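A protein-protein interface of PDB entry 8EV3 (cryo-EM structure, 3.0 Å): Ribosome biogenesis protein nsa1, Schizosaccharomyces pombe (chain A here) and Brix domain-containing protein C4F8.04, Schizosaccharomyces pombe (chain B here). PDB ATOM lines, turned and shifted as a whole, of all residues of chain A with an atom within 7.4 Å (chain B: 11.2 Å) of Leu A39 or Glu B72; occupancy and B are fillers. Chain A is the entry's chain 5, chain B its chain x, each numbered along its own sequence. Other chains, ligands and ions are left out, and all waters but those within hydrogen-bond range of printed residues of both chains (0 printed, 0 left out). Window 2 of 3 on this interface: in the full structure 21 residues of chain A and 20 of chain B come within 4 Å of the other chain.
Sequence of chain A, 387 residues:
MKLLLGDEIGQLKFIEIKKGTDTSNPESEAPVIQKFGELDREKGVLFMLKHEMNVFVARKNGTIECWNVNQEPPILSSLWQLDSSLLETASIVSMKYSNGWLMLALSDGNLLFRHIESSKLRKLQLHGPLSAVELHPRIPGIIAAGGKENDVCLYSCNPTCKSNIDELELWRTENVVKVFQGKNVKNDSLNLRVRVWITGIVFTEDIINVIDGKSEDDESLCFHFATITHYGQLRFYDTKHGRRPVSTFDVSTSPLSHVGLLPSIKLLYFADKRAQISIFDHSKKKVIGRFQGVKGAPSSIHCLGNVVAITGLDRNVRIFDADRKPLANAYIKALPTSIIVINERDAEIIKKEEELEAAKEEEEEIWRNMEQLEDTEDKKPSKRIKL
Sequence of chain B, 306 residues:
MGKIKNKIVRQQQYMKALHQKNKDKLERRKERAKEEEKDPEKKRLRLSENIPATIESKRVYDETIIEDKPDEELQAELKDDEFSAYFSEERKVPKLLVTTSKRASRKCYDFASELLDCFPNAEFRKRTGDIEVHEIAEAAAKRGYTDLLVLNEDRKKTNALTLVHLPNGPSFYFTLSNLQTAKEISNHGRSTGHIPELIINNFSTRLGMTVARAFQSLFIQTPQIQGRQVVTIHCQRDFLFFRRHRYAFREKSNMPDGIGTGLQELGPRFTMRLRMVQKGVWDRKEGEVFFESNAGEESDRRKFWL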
ATOM      1  N   ASP A   7     -16.568  23.102  -3.978  1.00  0.00           N
ATOM      2  CA  ASP A   7     -15.957  22.966  -2.667  1.00  0.00           C
ATOM      3  C   ASP A   7     -14.450  22.797  -2.797  1.00  0.00           C
ATOM      4  O   ASP A   7     -13.905  22.668  -3.895  1.00  0.00           O
ATOM      5  CB  ASP A   7     -16.560  21.781  -1.902  1.00  0.00           C
ATOM      6  CG  ASP A   7     -18.030  21.978  -1.590  1.00  0.00           C
ATOM      7  OD1 ASP A   7     -18.408  23.101  -1.203  1.00  0.00           O
ATOM      8  OD2 ASP A   7     -18.807  21.011  -1.726  1.00  0.00           O
ATOM      9  N   GLU A   8     -13.774  22.801  -1.647  1.00  0.00           N
ATOM     10  CA  GLU A   8     -12.328  22.617  -1.631  1.00  0.00           C
ATOM     11  C   GLU A   8     -11.916  21.210  -2.034  1.00  0.00           C
ATOM     12  O   GLU A   8     -10.754  20.999  -2.393  1.00  0.00           O
ATOM     13  CB  GLU A   8     -11.765  22.936  -0.247  1.00  0.00           C
ATOM     14  CG  GLU A   8     -12.327  24.194   0.381  1.00  0.00           C
ATOM     15  CD  GLU A   8     -11.296  24.951   1.195  1.00  0.00           C
ATOM     16  OE1 GLU A   8     -10.463  24.300   1.859  1.00  0.00           O
ATOM     17  OE2 GLU A   8     -11.315  26.198   1.168  1.00  0.00           O
ATOM     18  N   ILE A   9     -12.830  20.244  -1.977  1.00  0.00           N
ATOM     19  CA  ILE A   9     -12.517  18.870  -2.351  1.00  0.00           C
ATOM     20  C   ILE A   9     -12.918  18.645  -3.803  1.00  0.00           C
ATOM     21  O   ILE A   9     -12.905  17.513  -4.298  1.00  0.00           O
ATOM     22  CB  ILE A   9     -13.208  17.862  -1.416  1.00  0.00           C
ATOM     23  CG1 ILE A   9     -14.720  18.069  -1.430  1.00  0.00           C
ATOM     24  CG2 ILE A   9     -12.671  18.002  -0.005  1.00  0.00           C
ATOM     25  CD1 ILE A   9     -15.459  17.194  -0.448  1.00  0.00           C
ATOM     26  N   GLY A  10     -13.283  19.724  -4.492  1.00  0.00           N
ATOM     27  CA  GLY A  10     -13.510  19.685  -5.920  1.00  0.00           C
ATOM     28  C   GLY A  10     -14.873  19.211  -6.365  1.00  0.00           C
ATOM     29  O   GLY A  10     -15.086  19.060  -7.573  1.00  0.00           O
ATOM     30  N   GLN A  11     -15.802  18.972  -5.446  1.00  0.00           N
ATOM     31  CA  GLN A  11     -17.120  18.489  -5.827  1.00  0.00           C
ATOM     32  C   GLN A  11     -18.047  19.650  -6.161  1.00  0.00           C
ATOM     33  O   GLN A  11     -17.968  20.727  -5.565  1.00  0.00           O
ATOM     34  CB  GLN A  11     -17.732  17.633  -4.718  1.00  0.00           C
ATOM     35  CG  GLN A  11     -18.055  18.376  -3.442  1.00  0.00           C
ATOM     36  CD  GLN A  11     -18.667  17.472  -2.395  1.00  0.00           C
ATOM     37  OE1 GLN A  11     -19.158  16.390  -2.709  1.00  0.00           O
ATOM     38  NE2 GLN A  11     -18.643  17.910  -1.143  1.00  0.00           N
ATOM     39  N   LEU A  12     -18.922  19.420  -7.133  1.00  0.00           N
ATOM     40  CA  LEU A  12     -19.885  20.414  -7.585  1.00  0.00           C
ATOM     41  C   LEU A  12     -21.271  20.013  -7.104  1.00  0.00           C
ATOM     42  O   LEU A  12     -21.696  18.873  -7.312  1.00  0.00           O
ATOM     43  CB  LEU A  12     -19.873  20.541  -9.110  1.00  0.00           C
ATOM     44  CG  LEU A  12     -18.760  21.352  -9.777  1.00  0.00           C
ATOM     45  CD1 LEU A  12     -18.568  22.680  -9.075  1.00  0.00           C
ATOM     46  CD2 LEU A  12     -17.458  20.575  -9.817  1.00  0.00           C
ATOM     47  N   LYS A  35     -25.275  16.480  -6.219  1.00  0.00           N
ATOM     48  CA  LYS A  35     -23.828  16.607  -6.175  1.00  0.00           C
ATOM     49  C   LYS A  35     -23.170  15.683  -7.189  1.00  0.00           C
ATOM     50  O   LYS A  35     -23.649  14.579  -7.458  1.00  0.00           O
ATOM     51  CB  LYS A  35     -23.298  16.299  -4.774  1.00  0.00           C
ATOM     52  CG  LYS A  35     -23.727  14.951  -4.234  1.00  0.00           C
ATOM     53  CD  LYS A  35     -23.500  14.863  -2.736  1.00  0.00           C
ATOM     54  CE  LYS A  35     -22.031  15.016  -2.395  1.00  0.00           C
ATOM     55  NZ  LYS A  35     -21.190  14.016  -3.107  1.00  0.00           N
ATOM     56  N   PHE A  36     -22.064  16.151  -7.754  1.00  0.00           N
ATOM     57  CA  PHE A  36     -21.274  15.377  -8.703  1.00  0.00           C
ATOM     58  C   PHE A  36     -19.854  15.930  -8.687  1.00  0.00           C
ATOM     59  O   PHE A  36     -19.480  16.697  -7.795  1.00  0.00           O
ATOM     60  CB  PHE A  36     -21.899  15.416 -10.102  1.00  0.00           C
ATOM     61  CG  PHE A  36     -22.244  16.795 -10.576  1.00  0.00           C
ATOM     62  CD1 PHE A  36     -21.312  17.565 -11.248  1.00  0.00           C
ATOM     63  CD2 PHE A  36     -23.505  17.321 -10.356  1.00  0.00           C
ATOM     64  CE1 PHE A  36     -21.629  18.836 -11.685  1.00  0.00           C
ATOM     65  CE2 PHE A  36     -23.827  18.592 -10.792  1.00  0.00           C
ATOM     66  CZ  PHE A  36     -22.888  19.349 -11.456  1.00  0.00           C
ATOM     67  N   GLY A  37     -19.062  15.540  -9.672  1.00  0.00           N
ATOM     68  CA  GLY A  37     -17.686  15.978  -9.733  1.00  0.00           C
ATOM     69  C   GLY A  37     -16.759  15.115  -8.904  1.00  0.00           C
ATOM     70  O   GLY A  37     -17.104  14.029  -8.427  1.00  0.00           O
ATOM     71  N   GLU A  38     -15.546  15.626  -8.728  1.00  0.00           N
ATOM     72  CA  GLU A  38     -14.492  14.885  -8.060  1.00  0.00           C
ATOM     73  C   GLU A  38     -14.672  14.930  -6.544  1.00  0.00           C
ATOM     74  O   GLU A  38     -15.544  15.620  -6.011  1.00  0.00           O
ATOM     75  CB  GLU A  38     -13.126  15.442  -8.453  1.00  0.00           C
ATOM     76  CG  GLU A  38     -12.007  14.420  -8.443  1.00  0.00           C
ATOM     77  CD  GLU A  38     -10.697  15.008  -8.904  1.00  0.00           C
ATOM     78  OE1 GLU A  38     -10.645  16.238  -9.106  1.00  0.00           O
ATOM     79  OE2 GLU A  38      -9.722  14.244  -9.063  1.00  0.00           O
ATOM     80  N   LEU A  39     -13.835  14.168  -5.847  1.00  0.00           N
ATOM     81  CA  LEU A  39     -13.784  14.151  -4.391  1.00  0.00           C
ATOM     82  C   LEU A  39     -12.340  14.152  -3.912  1.00  0.00           C
ATOM     83  O   LEU A  39     -11.971  13.427  -2.985  1.00  0.00           O
ATOM     84  CB  LEU A  39     -14.539  12.950  -3.829  1.00  0.00           C
ATOM     85  CG  LEU A  39     -15.298  13.197  -2.526  1.00  0.00           C
ATOM     86  CD1 LEU A  39     -16.304  14.320  -2.703  1.00  0.00           C
ATOM     87  CD2 LEU A  39     -15.988  11.926  -2.060  1.00  0.00           C
ATOM     88  N   ASP A  40     -11.503  14.969  -4.545  1.00  0.00           N
ATOM     89  CA  ASP A  40     -10.082  15.045  -4.236  1.00  0.00           C
ATOM     90  C   ASP A  40      -9.716  16.478  -3.877  1.00  0.00           C
ATOM     91  O   ASP A  40     -10.128  17.419  -4.562  1.00  0.00           O
ATOM     92  CB  ASP A  40      -9.240  14.565  -5.422  1.00  0.00           C
ATOM     93  CG  ASP A  40      -7.772  14.427  -5.077  1.00  0.00           C
ATOM     94  OD1 ASP A  40      -7.426  14.525  -3.881  1.00  0.00           O
ATOM     95  OD2 ASP A  40      -6.962  14.220  -6.004  1.00  0.00           O
ATOM     96  N   ARG A  41      -8.938  16.636  -2.805  1.00  0.00           N
ATOM     97  CA  ARG A  41      -8.483  17.964  -2.409  1.00  0.00           C
ATOM     98  C   ARG A  41      -7.454  18.517  -3.387  1.00  0.00           C
ATOM     99  O   ARG A  41      -7.310  19.738  -3.508  1.00  0.00           O
ATOM    100  CB  ARG A  41      -7.903  17.913  -0.996  1.00  0.00           C
ATOM    101  CG  ARG A  41      -7.419  19.246  -0.457  1.00  0.00           C
ATOM    102  CD  ARG A  41      -8.582  20.102  -0.001  1.00  0.00           C
ATOM    103  NE  ARG A  41      -9.082  19.686   1.303  1.00  0.00           N
ATOM    104  CZ  ARG A  41      -8.768  20.277   2.447  1.00  0.00           C
ATOM    105  NH1 ARG A  41      -7.956  21.318   2.487  1.00  0.00           N
ATOM    106  NH2 ARG A  41      -9.285  19.811   3.580  1.00  0.00           N
ATOM    107  N   GLU A  42      -6.745  17.638  -4.099  1.00  0.00           N
ATOM    108  CA  GLU A  42      -5.682  18.086  -4.994  1.00  0.00           C
ATOM    109  C   GLU A  42      -6.218  18.925  -6.145  1.00  0.00           C
ATOM    110  O   GLU A  42      -5.473  19.720  -6.729  1.00  0.00           O
ATOM    111  CB  GLU A  42      -4.915  16.882  -5.536  1.00  0.00           C
ATOM    112  CG  GLU A  42      -3.689  16.514  -4.726  1.00  0.00           C
ATOM    113  CD  GLU A  42      -2.553  17.492  -4.928  1.00  0.00           C
ATOM    114  OE1 GLU A  42      -2.479  18.099  -6.016  1.00  0.00           O
ATOM    115  OE2 GLU A  42      -1.731  17.651  -4.002  1.00  0.00           O
ATOM    116  N   LYS A  43      -7.489  18.764  -6.493  1.00  0.00           N
ATOM    117  CA  LYS A  43      -8.098  19.486  -7.605  1.00  0.00           C
ATOM    118  C   LYS A  43      -9.380  20.173  -7.156  1.00  0.00           C
ATOM    119  O   LYS A  43     -10.431  20.064  -7.788  1.00  0.00           O
ATOM    120  CB  LYS A  43      -8.353  18.555  -8.786  1.00  0.00           C
ATOM    121  CG  LYS A  43      -7.518  17.285  -8.768  1.00  0.00           C
ATOM    122  CD  LYS A  43      -7.667  16.503 -10.061  1.00  0.00           C
ATOM    123  CE  LYS A  43      -6.775  15.273 -10.064  1.00  0.00           C
ATOM    124  NZ  LYS A  43      -6.989  14.435  -8.852  1.00  0.00           N
ATOM    125  N   ARG A  59     -10.031  24.606 -11.549  1.00  0.00           N
ATOM    126  CA  ARG A  59      -9.582  23.773 -10.446  1.00  0.00           C
ATOM    127  C   ARG A  59      -8.146  24.124 -10.083  1.00  0.00           C
ATOM    128  O   ARG A  59      -7.448  24.831 -10.811  1.00  0.00           O
ATOM    129  CB  ARG A  59      -9.707  22.287 -10.798  1.00  0.00           C
ATOM    130  CG  ARG A  59     -11.146  21.821 -10.916  1.00  0.00           C
ATOM    131  CD  ARG A  59     -11.246  20.312 -10.963  1.00  0.00           C
ATOM    132  NE  ARG A  59     -12.546  19.886 -11.466  1.00  0.00           N
ATOM    133  CZ  ARG A  59     -13.641  19.794 -10.726  1.00  0.00           C
ATOM    134  NH1 ARG A  59     -13.624  20.061  -9.431  1.00  0.00           N
ATOM    135  NH2 ARG A  59     -14.780  19.421 -11.298  1.00  0.00           N
ATOM    136  N   ALA A 334     -19.676  20.581   3.274  1.00  0.00           N
ATOM    137  CA  ALA A 334     -18.308  20.765   2.811  1.00  0.00           C
ATOM    138  C   ALA A 334     -17.950  22.243   2.723  1.00  0.00           C
ATOM    139  O   ALA A 334     -18.811  23.103   2.524  1.00  0.00           O
ATOM    140  CB  ALA A 334     -18.106  20.103   1.449  1.00  0.00           C
ATOM    141  N   ILE B  66     -22.749  16.338  13.855  1.00  0.00           N
ATOM    142  CA  ILE B  66     -22.355  15.134  13.131  1.00  0.00           C
ATOM    143  C   ILE B  66     -23.310  14.000  13.475  1.00  0.00           C
ATOM    144  O   ILE B  66     -24.050  14.072  14.461  1.00  0.00           O
ATOM    145  CB  ILE B  66     -20.902  14.740  13.444  1.00  0.00           C
ATOM    146  CG1 ILE B  66     -20.777  14.295  14.901  1.00  0.00           C
ATOM    147  CG2 ILE B  66     -19.961  15.892  13.145  1.00  0.00           C
ATOM    148  CD1 ILE B  66     -19.471  13.613  15.219  1.00  0.00           C
ATOM    149  N   GLU B  67     -23.297  12.949  12.664  1.00  0.00           N
ATOM    150  CA  GLU B  67     -24.145  11.786  12.865  1.00  0.00           C
ATOM    151  C   GLU B  67     -23.300  10.578  13.245  1.00  0.00           C
ATOM    152  O   GLU B  67     -22.087  10.542  13.024  1.00  0.00           O
ATOM    153  CB  GLU B  67     -24.964  11.480  11.604  1.00  0.00           C
ATOM    154  CG  GLU B  67     -26.051  12.502  11.237  1.00  0.00           C
ATOM    155  CD  GLU B  67     -27.027  12.821  12.368  1.00  0.00           C
ATOM    156  OE1 GLU B  67     -26.617  13.388  13.403  1.00  0.00           O
ATOM    157  OE2 GLU B  67     -28.223  12.496  12.217  1.00  0.00           O
ATOM    158  N   ASP B  68     -23.964   9.584  13.840  1.00  0.00           N
ATOM    159  CA  ASP B  68     -23.275   8.352  14.212  1.00  0.00           C
ATOM    160  C   ASP B  68     -22.787   7.599  12.982  1.00  0.00           C
ATOM    161  O   ASP B  68     -21.677   7.053  12.977  1.00  0.00           O
ATOM    162  CB  ASP B  68     -24.198   7.468  15.051  1.00  0.00           C
ATOM    163  CG  ASP B  68     -25.553   7.261  14.402  1.00  0.00           C
ATOM    164  OD1 ASP B  68     -25.863   7.983  13.429  1.00  0.00           O
ATOM    165  OD2 ASP B  68     -26.308   6.381  14.864  1.00  0.00           O
ATOM    166  N   LYS B  69     -23.602   7.555  11.933  1.00  0.00           N
ATOM    167  CA  LYS B  69     -23.218   6.845  10.724  1.00  0.00           C
ATOM    168  C   LYS B  69     -22.037   7.547  10.055  1.00  0.00           C
ATOM    169  O   LYS B  69     -21.942   8.777  10.093  1.00  0.00           O
ATOM    170  CB  LYS B  69     -24.397   6.761   9.754  1.00  0.00           C
ATOM    171  CG  LYS B  69     -24.908   8.110   9.282  1.00  0.00           C
ATOM    172  CD  LYS B  69     -25.982   7.959   8.221  1.00  0.00           C
ATOM    173  CE  LYS B  69     -26.561   9.311   7.834  1.00  0.00           C
ATOM    174  NZ  LYS B  69     -25.524  10.219   7.273  1.00  0.00           N
ATOM    175  N   PRO B  70     -21.119   6.797   9.451  1.00  0.00           N
ATOM    176  CA  PRO B  70     -19.995   7.432   8.757  1.00  0.00           C
ATOM    177  C   PRO B  70     -20.422   7.999   7.413  1.00  0.00           C
ATOM    178  O   PRO B  70     -21.176   7.376   6.661  1.00  0.00           O
ATOM    179  CB  PRO B  70     -18.995   6.283   8.586  1.00  0.00           C
ATOM    180  CG  PRO B  70     -19.843   5.062   8.535  1.00  0.00           C
ATOM    181  CD  PRO B  70     -21.042   5.327   9.409  1.00  0.00           C
ATOM    182  N   ASP B  71     -19.934   9.200   7.119  1.00  0.00           N
ATOM    183  CA  ASP B  71     -20.203   9.876   5.859  1.00  0.00           C
ATOM    184  C   ASP B  71     -18.896  10.073   5.106  1.00  0.00           C
ATOM    185  O   ASP B  71     -17.910  10.546   5.680  1.00  0.00           O
ATOM    186  CB  ASP B  71     -20.898  11.219   6.092  1.00  0.00           C
ATOM    187  CG  ASP B  71     -20.355  11.954   7.299  1.00  0.00           C
ATOM    188  OD1 ASP B  71     -19.575  11.351   8.064  1.00  0.00           O
ATOM    189  OD2 ASP B  71     -20.711  13.137   7.483  1.00  0.00           O
ATOM    190  N   GLU B  72     -18.895   9.705   3.824  1.00  0.00           N
ATOM    191  CA  GLU B  72     -17.669   9.766   3.035  1.00  0.00           C
ATOM    192  C   GLU B  72     -17.179  11.200   2.877  1.00  0.00           C
ATOM    193  O   GLU B  72     -15.970  11.460   2.932  1.00  0.00           O
ATOM    194  CB  GLU B  72     -17.900   9.118   1.669  1.00  0.00           C
ATOM    195  CG  GLU B  72     -16.909   9.532   0.594  1.00  0.00           C
ATOM    196  CD  GLU B  72     -15.667   8.662   0.574  1.00  0.00           C
ATOM    197  OE1 GLU B  72     -15.080   8.429   1.651  1.00  0.00           O
ATOM    198  OE2 GLU B  72     -15.277   8.209  -0.523  1.00  0.00           O
ATOM    199  N   GLU B  73     -18.102  12.146   2.684  1.00  0.00           N
ATOM    200  CA  GLU B  73     -17.705  13.533   2.459  1.00  0.00           C
ATOM    201  C   GLU B  73     -16.950  14.099   3.654  1.00  0.00           C
ATOM    202  O   GLU B  73     -15.939  14.792   3.486  1.00  0.00           O
ATOM    203  CB  GLU B  73     -18.935  14.384   2.152  1.00  0.00           C
ATOM    204  CG  GLU B  73     -18.614  15.775   1.642  1.00  0.00           C
ATOM    205  CD  GLU B  73     -19.809  16.702   1.704  1.00  0.00           C
ATOM    206  OE1 GLU B  73     -20.569  16.622   2.690  1.00  0.00           O
ATOM    207  OE2 GLU B  73     -19.993  17.507   0.768  1.00  0.00           O
ATOM    208  N   LEU B  74     -17.428  13.824   4.868  1.00  0.00           N
ATOM    209  CA  LEU B  74     -16.755  14.331   6.058  1.00  0.00           C
ATOM    210  C   LEU B  74     -15.369  13.714   6.205  1.00  0.00           C
ATOM    211  O   LEU B  74     -14.400  14.419   6.508  1.00  0.00           O
ATOM    212  CB  LEU B  74     -17.622  14.061   7.292  1.00  0.00           C
ATOM    213  CG  LEU B  74     -17.428  14.713   8.671  1.00  0.00           C
ATOM    214  CD1 LEU B  74     -18.407  14.097   9.654  1.00  0.00           C
ATOM    215  CD2 LEU B  74     -16.024  14.603   9.230  1.00  0.00           C
ATOM    216  N   GLN B  75     -15.251  12.404   5.983  1.00  0.00           N
ATOM    217  CA  GLN B  75     -13.957  11.748   6.117  1.00  0.00           C
ATOM    218  C   GLN B  75     -13.027  12.053   4.952  1.00  0.00           C
ATOM    219  O   GLN B  75     -11.809  11.905   5.093  1.00  0.00           O
ATOM    220  CB  GLN B  75     -14.139  10.237   6.259  1.00  0.00           C
ATOM    221  CG  GLN B  75     -14.119   9.750   7.700  1.00  0.00           C
ATOM    222  CD  GLN B  75     -15.510   9.582   8.279  1.00  0.00           C
ATOM    223  OE1 GLN B  75     -16.434   9.159   7.589  1.00  0.00           O
ATOM    224  NE2 GLN B  75     -15.663   9.915   9.555  1.00  0.00           N
ATOM    225  N   ALA B  76     -13.568  12.466   3.804  1.00  0.00           N
ATOM    226  CA  ALA B  76     -12.711  12.873   2.696  1.00  0.00           C
ATOM    227  C   ALA B  76     -12.093  14.239   2.946  1.00  0.00           C
ATOM    228  O   ALA B  76     -11.001  14.528   2.443  1.00  0.00           O
ATOM    229  CB  ALA B  76     -13.502  12.881   1.390  1.00  0.00           C
ATOM    230  N   GLU B  77     -12.775  15.089   3.711  1.00  0.00           N
ATOM    231  CA  GLU B  77     -12.268  16.423   3.999  1.00  0.00           C
ATOM    232  C   GLU B  77     -11.160  16.406   5.045  1.00  0.00           C
ATOM    233  O   GLU B  77     -10.277  17.269   5.018  1.00  0.00           O
ATOM    234  CB  GLU B  77     -13.416  17.321   4.457  1.00  0.00           C
ATOM    235  CG  GLU B  77     -13.043  18.773   4.641  1.00  0.00           C
ATOM    236  CD  GLU B  77     -14.257  19.669   4.748  1.00  0.00           C
ATOM    237  OE1 GLU B  77     -15.387  19.153   4.628  1.00  0.00           O
ATOM    238  OE2 GLU B  77     -14.080  20.888   4.954  1.00  0.00           O
ATOM    239  N   LEU B  78     -11.186  15.441   5.964  1.00  0.00           N
ATOM    240  CA  LEU B  78     -10.190  15.378   7.025  1.00  0.00           C
ATOM    241  C   LEU B  78      -8.914  14.660   6.613  1.00  0.00           C
ATOM    242  O   LEU B  78      -7.953  14.653   7.389  1.00  0.00           O
ATOM    243  CB  LEU B  78     -10.764  14.681   8.258  1.00  0.00           C
ATOM    244  CG  LEU B  78     -12.083  15.183   8.838  1.00  0.00           C
ATOM    245  CD1 LEU B  78     -12.559  14.222   9.909  1.00  0.00           C
ATOM    246  CD2 LEU B  78     -11.923  16.579   9.404  1.00  0.00           C
ATOM    247  N   LYS B  79      -8.875  14.056   5.429  1.00  0.00           N
ATOM    248  CA  LYS B  79      -7.719  13.278   5.008  1.00  0.00           C
ATOM    249  C   LYS B  79      -6.665  14.112   4.294  1.00  0.00           C
ATOM    250  O   LYS B  79      -5.594  13.586   3.974  1.00  0.00           O
ATOM    251  CB  LYS B  79      -8.160  12.124   4.104  1.00  0.00           C
ATOM    252  CG  LYS B  79      -8.418  12.516   2.662  1.00  0.00           C
ATOM    253  CD  LYS B  79      -7.440  11.825   1.727  1.00  0.00           C
ATOM    254  CE  LYS B  79      -7.870  11.953   0.276  1.00  0.00           C
ATOM    255  NZ  LYS B  79      -6.917  11.272  -0.642  1.00  0.00           N
ATOM    256  N   ASP B  80      -6.933  15.394   4.037  1.00  0.00           N
ATOM    257  CA  ASP B  80      -5.952  16.238   3.367  1.00  0.00           C
ATOM    258  C   ASP B  80      -5.891  17.644   3.956  1.00  0.00           C
ATOM    259  O   ASP B  80      -5.322  18.543   3.325  1.00  0.00           O
ATOM    260  CB  ASP B  80      -6.247  16.324   1.868  1.00  0.00           C
ATOM    261  CG  ASP B  80      -5.016  16.087   1.018  1.00  0.00           C
ATOM    262  OD1 ASP B  80      -3.893  16.223   1.547  1.00  0.00           O
ATOM    263  OD2 ASP B  80      -5.170  15.763  -0.179  1.00  0.00           O
ATOM    264  N   ASP B  81      -6.454  17.861   5.141  1.00  0.00           N
ATOM    265  CA  ASP B  81      -6.466  19.182   5.748  1.00  0.00           C
ATOM    266  C   ASP B  81      -5.149  19.423   6.483  1.00  0.00           C
ATOM    267  O   ASP B  81      -4.176  18.682   6.320  1.00  0.00           O
ATOM    268  CB  ASP B  81      -7.677  19.332   6.666  1.00  0.00           C
ATOM    269  CG  ASP B  81      -7.627  18.402   7.857  1.00  0.00           C
ATOM    270  OD1 ASP B  81      -6.881  17.403   7.808  1.00  0.00           O
ATOM    271  OD2 ASP B  81      -8.339  18.672   8.845  1.00  0.00           O
ATOM    272  N   ARG B 206     -19.921  20.240  13.910  1.00  0.00           N
ATOM    273  CA  ARG B 206     -18.832  20.211  12.940  1.00  0.00           C
ATOM    274  C   ARG B 206     -17.672  21.083  13.395  1.00  0.00           C
ATOM    275  O   ARG B 206     -16.505  20.700  13.256  1.00  0.00           O
ATOM    276  CB  ARG B 206     -19.338  20.662  11.571  1.00  0.00           C
ATOM    277  CG  ARG B 206     -18.263  20.727  10.504  1.00  0.00           C
ATOM    278  CD  ARG B 206     -17.876  19.343  10.029  1.00  0.00           C
ATOM    279  NE  ARG B 206     -16.702  19.373   9.166  1.00  0.00           N
ATOM    280  CZ  ARG B 206     -15.455  19.263   9.600  1.00  0.00           C
ATOM    281  NH1 ARG B 206     -15.182  19.119  10.884  1.00  0.00           N
ATOM    282  NH2 ARG B 206     -14.458  19.299   8.722  1.00  0.00           N
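Leu A39 touches Glu B72 (CD2 to CG, 3.7 Å). Arg A41 touches Asp B80 (CB to OD2, 3.6 Å). Asp B81 touches Arg A41 (CB to NH2, 3.5 Å). Ala A334 touches Glu B73 (CB to OE2, 3.3 Å). CA of Ala A334 touches OE1 of Glu B77, 3.8 Å away.
NH2 of Arg A41 sits at hydrogen-bond distance from O of Glu B77, at 3.1 Å. OE2 of Glu B73 sits close to NE2 of Gln A11, 2.4 Å away.
No residue of chain B comes within 4 Å of Ile A9. Of the printed residues of chain B, Gln A11 touches Glu B73 (2.4 Å). No residue of chain B comes within 4 Å of Gly A37. No residue of chain B comes within 4 Å of Glu A38. Leu A39 touches just one residue of chain B: Glu B72. No residue of chain B comes within 4 Å of Asp A40. Of the printed residues of chain B, Arg A41 touches Glu B77, Asp B80 and Asp B81. Of the printed residues of chain A, Glu B73 touches Gln A11 (2.4 Å) and Ala A334 (3.3 Å). Of the printed residues of chain A, Glu B77 touches Arg A41 and Ala A334. Of the printed residues of chain A, Asp B81 touches Arg A41 (3.5 Å). The nearest printed residue of chain A that does not touch Asp B81 is Glu A8 (7.5 Å).
NE2 of Gln A11 lies within hydrogen-bond range of OD2 of Asp A7, at 3.2 Å. The guanidinium group of Arg A41 lies within salt-bridge range of the side-chain carboxylate of Glu A8, at 3.9 Å. OE1 of Gln A11 is in hydrogen-bond range of NZ of Lys A35. The backbone carbonyl oxygen (O) of Glu A38 lies close to the backbone NH (N) of Gln A11 (3.4 Å).
Printed residues of chain B that touch a printed residue of chain A: Glu B72, Glu B73, Glu B77, Asp B80 and Asp B81. Hydrophobic or aromatic side chains of chain A within 4 Å of the printed part of chain B: Leu A39 and Ala A334. Along chain A the printed residues that touch a printed residue of chain B span positions 11 to 334. Among the printed residues, 7 pairs touch across the chains. Among the printed residues, no Asp or Glu carboxylate lies within 4 Å of a Lys or Arg side-chain nitrogen of the other chain.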
